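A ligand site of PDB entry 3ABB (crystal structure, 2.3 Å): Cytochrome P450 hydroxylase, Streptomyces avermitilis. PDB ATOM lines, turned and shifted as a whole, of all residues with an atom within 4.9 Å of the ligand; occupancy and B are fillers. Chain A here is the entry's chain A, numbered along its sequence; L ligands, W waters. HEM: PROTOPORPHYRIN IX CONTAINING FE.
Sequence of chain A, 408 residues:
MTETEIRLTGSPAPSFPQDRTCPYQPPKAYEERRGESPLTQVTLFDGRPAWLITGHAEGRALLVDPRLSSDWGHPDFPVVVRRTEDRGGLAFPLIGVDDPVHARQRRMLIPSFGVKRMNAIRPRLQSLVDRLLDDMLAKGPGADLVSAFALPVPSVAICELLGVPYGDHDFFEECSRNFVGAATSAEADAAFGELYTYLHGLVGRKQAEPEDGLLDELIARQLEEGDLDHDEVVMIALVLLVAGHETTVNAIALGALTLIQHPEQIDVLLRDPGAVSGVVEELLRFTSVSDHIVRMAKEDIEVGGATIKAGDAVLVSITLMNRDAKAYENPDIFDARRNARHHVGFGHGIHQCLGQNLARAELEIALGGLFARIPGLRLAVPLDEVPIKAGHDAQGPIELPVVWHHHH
The backbone carbonyl oxygen (O) of Ala 243 is in hydrogen-bond range of the side-chain hydroxyl (OG1) of Thr 247.
The backbone NH of Cys 353 lies within hydrogen-bond range of the backbone carbonyl oxygen of Phe 346.
NH1 of Arg 106 lies within hydrogen-bond range of O of Gln 352 (3.0 Å).
The side-chain sulfur (SG) of Cys 353 sits close to the backbone NH (N) of Gly 355.
The backbone carbonyl oxygen of Leu 94 sits close to a ring nitrogen (ND1) of His 351 (3.3 Å).
ND1 of His 351 is in hydrogen-bond range of NE2 of His 102 (3.3 Å).
The backbone carbonyl oxygen (O) of Gly 244 lies within hydrogen-bond range of the side-chain hydroxyl (OG1) of Thr 248 (2.8 Å).
Water W3 lies within hydrogen-bond range of an oxygen (O1A) of the ligand (2.8 Å), the backbone carbonyl oxygen (O) of Ile 95 (2.8 Å) and the guanidinium group (NH1) of Arg 295 (3.0 Å).
Water W4 bridges OE2 of Glu 362 (2.7 Å) and O of Gly 244 (2.8 Å).
The backbone carbonyl oxygen (O) of Leu 94 sits close to an oxygen (O1D) of the ligand, 3.4 Å away.
Ile 95 touches the ligand (CA to O1D, 3.4 Å).
Phe 113 touches the ligand.
Ile 158 touches the ligand (CD1 to CBC, 3.6 Å).
CD2 of Leu 161 touches CBC of the ligand, at 3.6 Å.
Leu 240 touches the ligand.
CB of Ala 243 touches C1D of the ligand, 3.6 Å away.
CA of Gly 244 touches C2C of the ligand (3.3 Å).
OG1 of Thr 247 touches C4B of the ligand, at 3.5 Å.
Thr 248 touches the ligand.
Ala 251 touches the ligand (CB to CBB, 3.5 Å).
CD2 of Leu 284 touches CBB of the ligand, 3.9 Å away.
Ser 290 touches the ligand.
Ile 293 touches the ligand (CD1 to O2A, 3.5 Å).
Ile 318 touches the ligand.
Gly 345 touches the ligand (O to CMB, 3.6 Å).
CE1 of Phe 346 touches C3B of the ligand, at 3.5 Å.
Gly 347 touches the ligand.
Ile 350 touches the ligand.
Gln 352 touches the ligand (O to CBD, 3.9 Å).
Gly 355 touches the ligand (CA to C3C, 3.5 Å).
CD2 of Leu 358 touches CBC of the ligand, at 3.96 Å.
Ala 359 touches the ligand.
Glu 362 touches the ligand (OE2 to CMC, 3.9 Å).
Of the 34 residues printed, 29 come within 4 Å of the ligand.
O2A of the ligand is in salt-bridge range of NH2 of Arg 295.
The guanidinium group (NH1) of Arg 106 is in salt-bridge range of an oxygen (O2D) of the ligand, 2.7 Å away.
An iron atom (FE) of the ligand is bound by the side-chain sulfur (SG) of Cys 353 (2.4 Å).
A ring nitrogen (NE2) of His 102 lies within hydrogen-bond range of an oxygen (O2D) of the ligand (2.5 Å).
ND1 of His 351 sits at hydrogen-bond distance from O1D of the ligand (2.6 Å).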
ATOM      1  N   LEU A  94      26.265   6.156  22.584  1.00  0.00           N
ATOM      2  CA  LEU A  94      25.389   7.314  22.435  1.00  0.00           C
ATOM      3  C   LEU A  94      25.805   8.288  21.329  1.00  0.00           C
ATOM      4  O   LEU A  94      25.232   8.282  20.243  1.00  0.00           O
ATOM      5  CB  LEU A  94      25.274   8.072  23.751  1.00  0.00           C
ATOM      6  CG  LEU A  94      24.628   7.319  24.867  1.00  0.00           C
ATOM      7  CD1 LEU A  94      25.064   7.920  26.179  1.00  0.00           C
ATOM      8  CD2 LEU A  94      23.149   7.604  24.615  1.00  0.00           C
ATOM      9  N   ILE A  95      26.837   9.078  21.608  1.00  0.00           N
ATOM     10  CA  ILE A  95      27.188  10.219  20.811  1.00  0.00           C
ATOM     11  C   ILE A  95      27.893   9.769  19.551  1.00  0.00           C
ATOM     12  O   ILE A  95      27.880  10.519  18.548  1.00  0.00           O
ATOM     13  CB  ILE A  95      28.023  11.209  21.622  1.00  0.00           C
ATOM     14  CG1 ILE A  95      28.163  12.559  20.880  1.00  0.00           C
ATOM     15  CG2 ILE A  95      29.414  10.667  21.896  1.00  0.00           C
ATOM     16  CD1 ILE A  95      28.458  13.764  21.847  1.00  0.00           C
ATOM     17  N   HIS A 102      22.116   3.490  19.083  1.00  0.00           N
ATOM     18  CA  HIS A 102      21.819   4.781  19.674  1.00  0.00           C
ATOM     19  C   HIS A 102      20.527   4.791  20.501  1.00  0.00           C
ATOM     20  O   HIS A 102      20.532   5.176  21.669  1.00  0.00           O
ATOM     21  CB  HIS A 102      21.789   5.910  18.616  1.00  0.00           C
ATOM     22  CG  HIS A 102      21.469   7.235  19.242  1.00  0.00           C
ATOM     23  ND1 HIS A 102      20.252   7.848  19.095  1.00  0.00           N
ATOM     24  CD2 HIS A 102      22.172   8.005  20.119  1.00  0.00           C
ATOM     25  CE1 HIS A 102      20.238   8.989  19.797  1.00  0.00           C
ATOM     26  NE2 HIS A 102      21.387   9.102  20.431  1.00  0.00           N
ATOM     27  N   ARG A 106      20.227   5.191  24.613  1.00  0.00           N
ATOM     28  CA  ARG A 106      19.573   6.365  25.104  1.00  0.00           C
ATOM     29  C   ARG A 106      18.274   6.072  25.893  1.00  0.00           C
ATOM     30  O   ARG A 106      17.975   6.706  26.968  1.00  0.00           O
ATOM     31  CB  ARG A 106      19.335   7.308  23.934  1.00  0.00           C
ATOM     32  CG  ARG A 106      18.708   8.656  24.406  1.00  0.00           C
ATOM     33  CD  ARG A 106      18.872   9.763  23.320  1.00  0.00           C
ATOM     34  NE  ARG A 106      18.156  10.948  23.744  1.00  0.00           N
ATOM     35  CZ  ARG A 106      18.640  12.163  23.622  1.00  0.00           C
ATOM     36  NH1 ARG A 106      19.821  12.350  23.064  1.00  0.00           N
ATOM     37  NH2 ARG A 106      17.884  13.169  23.962  1.00  0.00           N
ATOM     38  N   PHE A 113      17.272  11.046  33.937  1.00  0.00           N
ATOM     39  CA  PHE A 113      17.486  12.468  33.795  1.00  0.00           C
ATOM     40  C   PHE A 113      16.176  13.164  34.078  1.00  0.00           C
ATOM     41  O   PHE A 113      15.963  14.278  33.571  1.00  0.00           O
ATOM     42  CB  PHE A 113      17.974  12.850  32.381  1.00  0.00           C
ATOM     43  CG  PHE A 113      19.398  12.525  32.157  1.00  0.00           C
ATOM     44  CD1 PHE A 113      20.397  13.440  32.495  1.00  0.00           C
ATOM     45  CD2 PHE A 113      19.770  11.265  31.742  1.00  0.00           C
ATOM     46  CE1 PHE A 113      21.711  13.105  32.338  1.00  0.00           C
ATOM     47  CE2 PHE A 113      21.118  10.932  31.574  1.00  0.00           C
ATOM     48  CZ  PHE A 113      22.087  11.853  31.879  1.00  0.00           C
ATOM     49  N   ILE A 158      28.244  15.215  38.173  1.00  0.00           N
ATOM     50  CA  ILE A 158      28.334  13.867  37.624  1.00  0.00           C
ATOM     51  C   ILE A 158      28.413  12.801  38.742  1.00  0.00           C
ATOM     52  O   ILE A 158      27.801  11.744  38.589  1.00  0.00           O
ATOM     53  CB  ILE A 158      29.491  13.707  36.619  1.00  0.00           C
ATOM     54  CG1 ILE A 158      29.202  14.533  35.352  1.00  0.00           C
ATOM     55  CG2 ILE A 158      29.734  12.214  36.308  1.00  0.00           C
ATOM     56  CD1 ILE A 158      28.043  14.066  34.471  1.00  0.00           C
ATOM     57  N   LEU A 161      24.813  12.499  39.967  1.00  0.00           N
ATOM     58  CA  LEU A 161      24.054  11.853  38.902  1.00  0.00           C
ATOM     59  C   LEU A 161      24.278  10.332  38.885  1.00  0.00           C
ATOM     60  O   LEU A 161      23.314   9.571  38.922  1.00  0.00           O
ATOM     61  CB  LEU A 161      24.465  12.383  37.538  1.00  0.00           C
ATOM     62  CG  LEU A 161      23.745  11.721  36.360  1.00  0.00           C
ATOM     63  CD1 LEU A 161      22.252  12.008  36.425  1.00  0.00           C
ATOM     64  CD2 LEU A 161      24.316  12.263  35.029  1.00  0.00           C
ATOM     65  N   VAL A 239      31.258   8.306  28.881  1.00  0.00           N
ATOM     66  CA  VAL A 239      30.659   9.305  27.926  1.00  0.00           C
ATOM     67  C   VAL A 239      29.880  10.402  28.653  1.00  0.00           C
ATOM     68  O   VAL A 239      30.018  11.560  28.306  1.00  0.00           O
ATOM     69  CB  VAL A 239      29.726   8.640  26.898  1.00  0.00           C
ATOM     70  CG1 VAL A 239      29.129   9.655  25.974  1.00  0.00           C
ATOM     71  CG2 VAL A 239      30.550   7.718  26.032  1.00  0.00           C
ATOM     72  N   LEU A 240      29.060  10.046  29.658  1.00  0.00           N
ATOM     73  CA  LEU A 240      28.372  11.053  30.427  1.00  0.00           C
ATOM     74  C   LEU A 240      29.404  12.064  31.067  1.00  0.00           C
ATOM     75  O   LEU A 240      29.209  13.272  31.028  1.00  0.00           O
ATOM     76  CB  LEU A 240      27.443  10.433  31.492  1.00  0.00           C
ATOM     77  CG  LEU A 240      26.315   9.636  30.789  1.00  0.00           C
ATOM     78  CD1 LEU A 240      25.515   8.824  31.777  1.00  0.00           C
ATOM     79  CD2 LEU A 240      25.399  10.563  30.010  1.00  0.00           C
ATOM     80  N   ALA A 243      31.295  14.135  28.144  1.00  0.00           N
ATOM     81  CA  ALA A 243      30.356  15.040  27.478  1.00  0.00           C
ATOM     82  C   ALA A 243      29.943  16.145  28.423  1.00  0.00           C
ATOM     83  O   ALA A 243      29.714  17.256  27.978  1.00  0.00           O
ATOM     84  CB  ALA A 243      29.123  14.300  26.977  1.00  0.00           C
ATOM     85  N   GLY A 244      29.904  15.860  29.723  1.00  0.00           N
ATOM     86  CA  GLY A 244      29.292  16.787  30.649  1.00  0.00           C
ATOM     87  C   GLY A 244      30.233  17.577  31.548  1.00  0.00           C
ATOM     88  O   GLY A 244      29.801  18.456  32.322  1.00  0.00           O
ATOM     89  N   THR A 247      32.556  20.756  28.863  1.00  0.00           N
ATOM     90  CA  THR A 247      31.678  21.757  28.246  1.00  0.00           C
ATOM     91  C   THR A 247      31.013  22.627  29.312  1.00  0.00           C
ATOM     92  O   THR A 247      30.840  23.824  29.087  1.00  0.00           O
ATOM     93  CB  THR A 247      30.553  21.089  27.465  1.00  0.00           C
ATOM     94  OG1 THR A 247      29.969  20.146  28.376  1.00  0.00           O
ATOM     95  CG2 THR A 247      31.071  20.364  26.298  1.00  0.00           C
ATOM     96  N   THR A 248      30.626  22.024  30.425  1.00  0.00           N
ATOM     97  CA  THR A 248      29.958  22.731  31.495  1.00  0.00           C
ATOM     98  C   THR A 248      30.946  23.609  32.191  1.00  0.00           C
ATOM     99  O   THR A 248      30.615  24.670  32.566  1.00  0.00           O
ATOM    100  CB  THR A 248      29.274  21.779  32.551  1.00  0.00           C
ATOM    101  OG1 THR A 248      28.443  20.839  31.890  1.00  0.00           O
ATOM    102  CG2 THR A 248      28.385  22.525  33.505  1.00  0.00           C
ATOM    103  N   ALA A 251      31.139  26.477  30.040  1.00  0.00           N
ATOM    104  CA  ALA A 251      29.910  27.242  29.981  1.00  0.00           C
ATOM    105  C   ALA A 251      29.843  28.074  31.260  1.00  0.00           C
ATOM    106  O   ALA A 251      29.438  29.224  31.216  1.00  0.00           O
ATOM    107  CB  ALA A 251      28.694  26.308  29.822  1.00  0.00           C
ATOM    108  N   LEU A 284      23.954  30.392  26.640  1.00  0.00           N
ATOM    109  CA  LEU A 284      24.139  29.195  25.842  1.00  0.00           C
ATOM    110  C   LEU A 284      24.200  29.579  24.374  1.00  0.00           C
ATOM    111  O   LEU A 284      25.063  29.107  23.687  1.00  0.00           O
ATOM    112  CB  LEU A 284      23.039  28.100  26.111  1.00  0.00           C
ATOM    113  CG  LEU A 284      23.195  27.454  27.521  1.00  0.00           C
ATOM    114  CD1 LEU A 284      21.890  26.865  28.077  1.00  0.00           C
ATOM    115  CD2 LEU A 284      24.357  26.374  27.566  1.00  0.00           C
ATOM    116  N   VAL A 289      29.452  27.292  23.466  1.00  0.00           N
ATOM    117  CA  VAL A 289      30.625  26.539  23.977  1.00  0.00           C
ATOM    118  C   VAL A 289      31.011  25.246  23.171  1.00  0.00           C
ATOM    119  O   VAL A 289      32.223  25.018  22.937  1.00  0.00           O
ATOM    120  CB  VAL A 289      30.392  26.214  25.473  1.00  0.00           C
ATOM    121  CG1 VAL A 289      31.243  25.142  25.881  1.00  0.00           C
ATOM    122  CG2 VAL A 289      30.707  27.449  26.251  1.00  0.00           C
ATOM    123  N   SER A 290      30.017  24.416  22.779  1.00  0.00           N
ATOM    124  CA  SER A 290      30.262  23.413  21.719  1.00  0.00           C
ATOM    125  C   SER A 290      30.043  24.178  20.433  1.00  0.00           C
ATOM    126  O   SER A 290      28.928  24.656  20.153  1.00  0.00           O
ATOM    127  CB  SER A 290      29.226  22.292  21.734  1.00  0.00           C
ATOM    128  OG  SER A 290      28.910  22.014  23.071  1.00  0.00           O
ATOM    129  N   ILE A 293      29.299  20.421  15.660  1.00  0.00           N
ATOM    130  CA  ILE A 293      29.212  18.976  15.771  1.00  0.00           C
ATOM    131  C   ILE A 293      29.361  18.329  14.359  1.00  0.00           C
ATOM    132  O   ILE A 293      29.169  18.982  13.311  1.00  0.00           O
ATOM    133  CB  ILE A 293      27.898  18.625  16.422  1.00  0.00           C
ATOM    134  CG1 ILE A 293      26.738  19.041  15.513  1.00  0.00           C
ATOM    135  CG2 ILE A 293      27.822  19.284  17.875  1.00  0.00           C
ATOM    136  CD1 ILE A 293      25.371  19.046  16.224  1.00  0.00           C
ATOM    137  N   ARG A 295      29.057  15.228  11.363  1.00  0.00           N
ATOM    138  CA  ARG A 295      28.224  14.203  10.801  1.00  0.00           C
ATOM    139  C   ARG A 295      28.792  13.707   9.471  1.00  0.00           C
ATOM    140  O   ARG A 295      29.723  14.304   8.881  1.00  0.00           O
ATOM    141  CB  ARG A 295      26.791  14.716  10.573  1.00  0.00           C
ATOM    142  CG  ARG A 295      26.052  15.261  11.856  1.00  0.00           C
ATOM    143  CD  ARG A 295      25.596  14.110  12.706  1.00  0.00           C
ATOM    144  NE  ARG A 295      24.650  14.526  13.740  1.00  0.00           N
ATOM    145  CZ  ARG A 295      25.031  14.920  14.972  1.00  0.00           C
ATOM    146  NH1 ARG A 295      26.339  15.025  15.294  1.00  0.00           N
ATOM    147  NH2 ARG A 295      24.067  15.228  15.868  1.00  0.00           N
ATOM    148  N   ILE A 318      27.125  25.091  15.380  1.00  0.00           N
ATOM    149  CA  ILE A 318      26.347  25.595  16.471  1.00  0.00           C
ATOM    150  C   ILE A 318      26.521  27.118  16.680  1.00  0.00           C
ATOM    151  O   ILE A 318      25.505  27.869  16.764  1.00  0.00           O
ATOM    152  CB  ILE A 318      26.626  24.798  17.756  1.00  0.00           C
ATOM    153  CG1 ILE A 318      25.887  23.426  17.621  1.00  0.00           C
ATOM    154  CG2 ILE A 318      26.084  25.594  18.966  1.00  0.00           C
ATOM    155  CD1 ILE A 318      26.322  22.363  18.564  1.00  0.00           C
ATOM    156  N   VAL A 344      20.646  26.351  19.630  1.00  0.00           N
ATOM    157  CA  VAL A 344      21.160  25.012  19.477  1.00  0.00           C
ATOM    158  C   VAL A 344      22.436  24.834  20.299  1.00  0.00           C
ATOM    159  O   VAL A 344      23.236  23.986  19.962  1.00  0.00           O
ATOM    160  CB  VAL A 344      21.333  24.630  17.997  1.00  0.00           C
ATOM    161  CG1 VAL A 344      19.934  24.468  17.285  1.00  0.00           C
ATOM    162  CG2 VAL A 344      22.138  25.666  17.289  1.00  0.00           C
ATOM    163  N   GLY A 345      22.591  25.579  21.404  1.00  0.00           N
ATOM    164  CA  GLY A 345      23.793  25.402  22.297  1.00  0.00           C
ATOM    165  C   GLY A 345      23.854  23.969  22.805  1.00  0.00           C
ATOM    166  O   GLY A 345      24.949  23.438  22.997  1.00  0.00           O
ATOM    167  N   PHE A 346      22.684  23.323  22.954  1.00  0.00           N
ATOM    168  CA  PHE A 346      22.607  21.905  23.353  1.00  0.00           C
ATOM    169  C   PHE A 346      22.324  20.978  22.134  1.00  0.00           C
ATOM    170  O   PHE A 346      21.868  19.806  22.302  1.00  0.00           O
ATOM    171  CB  PHE A 346      21.517  21.641  24.387  1.00  0.00           C
ATOM    172  CG  PHE A 346      21.828  22.212  25.739  1.00  0.00           C
ATOM    173  CD1 PHE A 346      22.985  21.851  26.420  1.00  0.00           C
ATOM    174  CD2 PHE A 346      20.908  23.071  26.363  1.00  0.00           C
ATOM    175  CE1 PHE A 346      23.279  22.374  27.707  1.00  0.00           C
ATOM    176  CE2 PHE A 346      21.171  23.550  27.664  1.00  0.00           C
ATOM    177  CZ  PHE A 346      22.387  23.202  28.320  1.00  0.00           C
ATOM    178  N   GLY A 347      22.605  21.488  20.942  1.00  0.00           N
ATOM    179  CA  GLY A 347      22.371  20.625  19.784  1.00  0.00           C
ATOM    180  C   GLY A 347      20.888  20.530  19.490  1.00  0.00           C
ATOM    181  O   GLY A 347      20.108  21.399  19.946  1.00  0.00           O
ATOM    182  N   ILE A 350      18.208  14.144  16.959  1.00  0.00           N
ATOM    183  CA  ILE A 350      18.568  12.784  17.345  1.00  0.00           C
ATOM    184  C   ILE A 350      19.525  12.697  18.524  1.00  0.00           C
ATOM    185  O   ILE A 350      19.297  11.861  19.415  1.00  0.00           O
ATOM    186  CB  ILE A 350      19.127  12.044  16.109  1.00  0.00           C
ATOM    187  CG1 ILE A 350      18.059  12.015  15.014  1.00  0.00           C
ATOM    188  CG2 ILE A 350      19.644  10.593  16.434  1.00  0.00           C
ATOM    189  CD1 ILE A 350      18.556  11.429  13.700  1.00  0.00           C
ATOM    190  N   HIS A 351      20.602  13.501  18.541  1.00  0.00           N
ATOM    191  CA  HIS A 351      21.649  13.387  19.551  1.00  0.00           C
ATOM    192  C   HIS A 351      21.674  14.607  20.452  1.00  0.00           C
ATOM    193  O   HIS A 351      22.695  14.910  21.057  1.00  0.00           O
ATOM    194  CB  HIS A 351      23.031  13.272  18.886  1.00  0.00           C
ATOM    195  CG  HIS A 351      23.245  11.964  18.199  1.00  0.00           C
ATOM    196  ND1 HIS A 351      23.749  10.853  18.854  1.00  0.00           N
ATOM    197  CD2 HIS A 351      23.023  11.576  16.918  1.00  0.00           C
ATOM    198  CE1 HIS A 351      23.816   9.845  18.001  1.00  0.00           C
ATOM    199  NE2 HIS A 351      23.369  10.248  16.826  1.00  0.00           N
ATOM    200  N   GLN A 352      20.588  15.361  20.526  1.00  0.00           N
ATOM    201  CA  GLN A 352      20.684  16.596  21.295  1.00  0.00           C
ATOM    202  C   GLN A 352      21.033  16.271  22.725  1.00  0.00           C
ATOM    203  O   GLN A 352      20.695  15.171  23.247  1.00  0.00           O
ATOM    204  CB  GLN A 352      19.375  17.378  21.259  1.00  0.00           C
ATOM    205  CG  GLN A 352      18.181  16.615  21.823  1.00  0.00           C
ATOM    206  CD  GLN A 352      16.922  17.469  21.863  1.00  0.00           C
ATOM    207  OE1 GLN A 352      16.288  17.618  22.932  1.00  0.00           O
ATOM    208  NE2 GLN A 352      16.555  18.048  20.711  1.00  0.00           N
ATOM    209  N   CYS A 353      21.610  17.237  23.378  1.00  0.00           N
ATOM    210  CA  CYS A 353      22.152  16.953  24.718  1.00  0.00           C
ATOM    211  C   CYS A 353      21.179  16.286  25.693  1.00  0.00           C
ATOM    212  O   CYS A 353      20.121  16.850  26.061  1.00  0.00           O
ATOM    213  CB  CYS A 353      22.629  18.251  25.356  1.00  0.00           C
ATOM    214  SG  CYS A 353      23.499  18.010  26.884  1.00  0.00           S
ATOM    215  N   LEU A 354      21.589  15.132  26.173  1.00  0.00           N
ATOM    216  CA  LEU A 354      20.808  14.380  27.114  1.00  0.00           C
ATOM    217  C   LEU A 354      20.950  14.990  28.517  1.00  0.00           C
ATOM    218  O   LEU A 354      20.036  14.857  29.347  1.00  0.00           O
ATOM    219  CB  LEU A 354      21.422  12.987  27.261  1.00  0.00           C
ATOM    220  CG  LEU A 354      20.567  11.727  27.403  1.00  0.00           C
ATOM    221  CD1 LEU A 354      21.283  10.709  28.287  1.00  0.00           C
ATOM    222  CD2 LEU A 354      19.122  11.884  27.820  1.00  0.00           C
ATOM    223  N   GLY A 355      22.104  15.577  28.786  1.00  0.00           N
ATOM    224  CA  GLY A 355      22.296  16.053  30.166  1.00  0.00           C
ATOM    225  C   GLY A 355      21.902  17.508  30.357  1.00  0.00           C
ATOM    226  O   GLY A 355      22.274  18.096  31.385  1.00  0.00           O
ATOM    227  N   LEU A 358      20.471  18.940  33.604  1.00  0.00           N
ATOM    228  CA  LEU A 358      21.485  18.967  34.658  1.00  0.00           C
ATOM    229  C   LEU A 358      22.401  20.223  34.446  1.00  0.00           C
ATOM    230  O   LEU A 358      22.662  20.993  35.377  1.00  0.00           O
ATOM    231  CB  LEU A 358      22.268  17.674  34.703  1.00  0.00           C
ATOM    232  CG  LEU A 358      23.356  17.656  35.769  1.00  0.00           C
ATOM    233  CD1 LEU A 358      22.735  18.046  37.181  1.00  0.00           C
ATOM    234  CD2 LEU A 358      24.114  16.307  35.808  1.00  0.00           C
ATOM    235  N   ALA A 359      22.784  20.482  33.193  1.00  0.00           N
ATOM    236  CA  ALA A 359      23.701  21.557  32.883  1.00  0.00           C
ATOM    237  C   ALA A 359      23.038  22.881  33.194  1.00  0.00           C
ATOM    238  O   ALA A 359      23.699  23.764  33.827  1.00  0.00           O
ATOM    239  CB  ALA A 359      24.126  21.505  31.467  1.00  0.00           C
ATOM    240  N   GLU A 362      23.271  23.454  36.760  1.00  0.00           N
ATOM    241  CA  GLU A 362      24.586  23.825  37.220  1.00  0.00           C
ATOM    242  C   GLU A 362      24.809  25.314  36.922  1.00  0.00           C
ATOM    243  O   GLU A 362      25.336  26.073  37.759  1.00  0.00           O
ATOM    244  CB  GLU A 362      25.642  22.951  36.554  1.00  0.00           C
ATOM    245  CG  GLU A 362      25.574  21.434  36.914  1.00  0.00           C
ATOM    246  CD  GLU A 362      26.637  20.631  36.188  1.00  0.00           C
ATOM    247  OE1 GLU A 362      27.840  20.973  36.368  1.00  0.00           O
ATOM    248  OE2 GLU A 362      26.302  19.635  35.486  1.00  0.00           O
ATOM    249  N   LEU A 363      24.371  25.737  35.742  1.00  0.00           N
ATOM    250  CA  LEU A 363      24.589  27.086  35.298  1.00  0.00           C
ATOM    251  C   LEU A 363      23.806  28.082  36.093  1.00  0.00           C
ATOM    252  O   LEU A 363      24.352  29.044  36.593  1.00  0.00           O
ATOM    253  CB  LEU A 363      24.295  27.195  33.803  1.00  0.00           C
ATOM    254  CG  LEU A 363      25.396  26.658  32.903  1.00  0.00           C
ATOM    255  CD1 LEU A 363      24.851  26.520  31.477  1.00  0.00           C
ATOM    256  CD2 LEU A 363      26.592  27.624  32.934  1.00  0.00           C
HETATM  257  CHA HEM L   1      25.211  15.807  23.430  1.00  0.00           C
HETATM  258  CHB HEM L   1      26.297  20.427  24.532  1.00  0.00           C
HETATM  259  CHC HEM L   1      26.383  19.222  29.182  1.00  0.00           C
HETATM  260  CHD HEM L   1      25.750  14.574  28.113  1.00  0.00           C
HETATM  261  C1A HEM L   1      25.438  17.163  23.311  1.00  0.00           C
HETATM  262  C2A HEM L   1      25.454  17.904  22.086  1.00  0.00           C
HETATM  263  C3A HEM L   1      25.758  19.183  22.379  1.00  0.00           C
HETATM  264  C4A HEM L   1      25.940  19.272  23.820  1.00  0.00           C
HETATM  265  CMA HEM L   1      25.905  20.366  21.404  1.00  0.00           C
HETATM  266  CAA HEM L   1      25.183  17.367  20.680  1.00  0.00           C
HETATM  267  CBA HEM L   1      26.232  16.376  20.157  1.00  0.00           C
HETATM  268  CGA HEM L   1      25.933  15.954  18.722  1.00  0.00           C
HETATM  269  O1A HEM L   1      26.867  15.369  18.132  1.00  0.00           O
HETATM  270  O2A HEM L   1      24.794  16.230  18.133  1.00  0.00           O
HETATM  271  C1B HEM L   1      26.417  20.542  25.891  1.00  0.00           C
HETATM  272  C2B HEM L   1      26.663  21.732  26.646  1.00  0.00           C
HETATM  273  C3B HEM L   1      26.680  21.395  27.937  1.00  0.00           C
HETATM  274  C4B HEM L   1      26.468  19.947  28.020  1.00  0.00           C
HETATM  275  CMB HEM L   1      26.833  23.167  26.039  1.00  0.00           C
HETATM  276  CAB HEM L   1      26.919  22.296  29.193  1.00  0.00           C
HETATM  277  CBB HEM L   1      26.538  23.589  29.222  1.00  0.00           C
HETATM  278  C1C HEM L   1      26.152  17.895  29.352  1.00  0.00           C
HETATM  279  C2C HEM L   1      26.035  17.196  30.607  1.00  0.00           C
HETATM  280  C3C HEM L   1      25.833  15.899  30.284  1.00  0.00           C
HETATM  281  C4C HEM L   1      25.880  15.745  28.828  1.00  0.00           C
HETATM  282  CMC HEM L   1      26.055  17.813  32.042  1.00  0.00           C
HETATM  283  CAC HEM L   1      25.703  14.682  31.190  1.00  0.00           C
HETATM  284  CBC HEM L   1      25.169  14.599  32.392  1.00  0.00           C
HETATM  285  C1D HEM L   1      25.564  14.466  26.768  1.00  0.00           C
HETATM  286  C2D HEM L   1      25.336  13.223  26.074  1.00  0.00           C
HETATM  287  C3D HEM L   1      25.169  13.578  24.587  1.00  0.00           C
HETATM  288  C4D HEM L   1      25.338  15.033  24.556  1.00  0.00           C
HETATM  289  CMD HEM L   1      25.291  11.843  26.700  1.00  0.00           C
HETATM  290  CAD HEM L   1      24.864  12.588  23.437  1.00  0.00           C
HETATM  291  CBD HEM L   1      23.330  12.307  23.453  1.00  0.00           C
HETATM  292  CGD HEM L   1      23.054  11.421  22.251  1.00  0.00           C
HETATM  293  O1D HEM L   1      24.022  11.187  21.459  1.00  0.00           O
HETATM  294  O2D HEM L   1      21.899  10.942  22.069  1.00  0.00           O
HETATM  295  NA  HEM L   1      25.759  18.001  24.358  1.00  0.00           N
HETATM  296  NB  HEM L   1      26.306  19.475  26.747  1.00  0.00           N
HETATM  297  NC  HEM L   1      26.058  16.968  28.290  1.00  0.00           N
HETATM  298  ND  HEM L   1      25.561  15.518  25.850  1.00  0.00           N
HETATM  299 FE   HEM L   1      25.756  17.534  26.381  1.00  0.00          FE
HETATM  300  O   HOH W   1      28.472  17.365  25.595  1.00  0.00           O
HETATM  301  O   HOH W   2      22.266  17.501  18.321  1.00  0.00           O
HETATM  302  O   HOH W   3      26.856  12.758  17.219  1.00  0.00           O
HETATM  303  O   HOH W   4      28.325  18.077  34.656  1.00  0.00           O
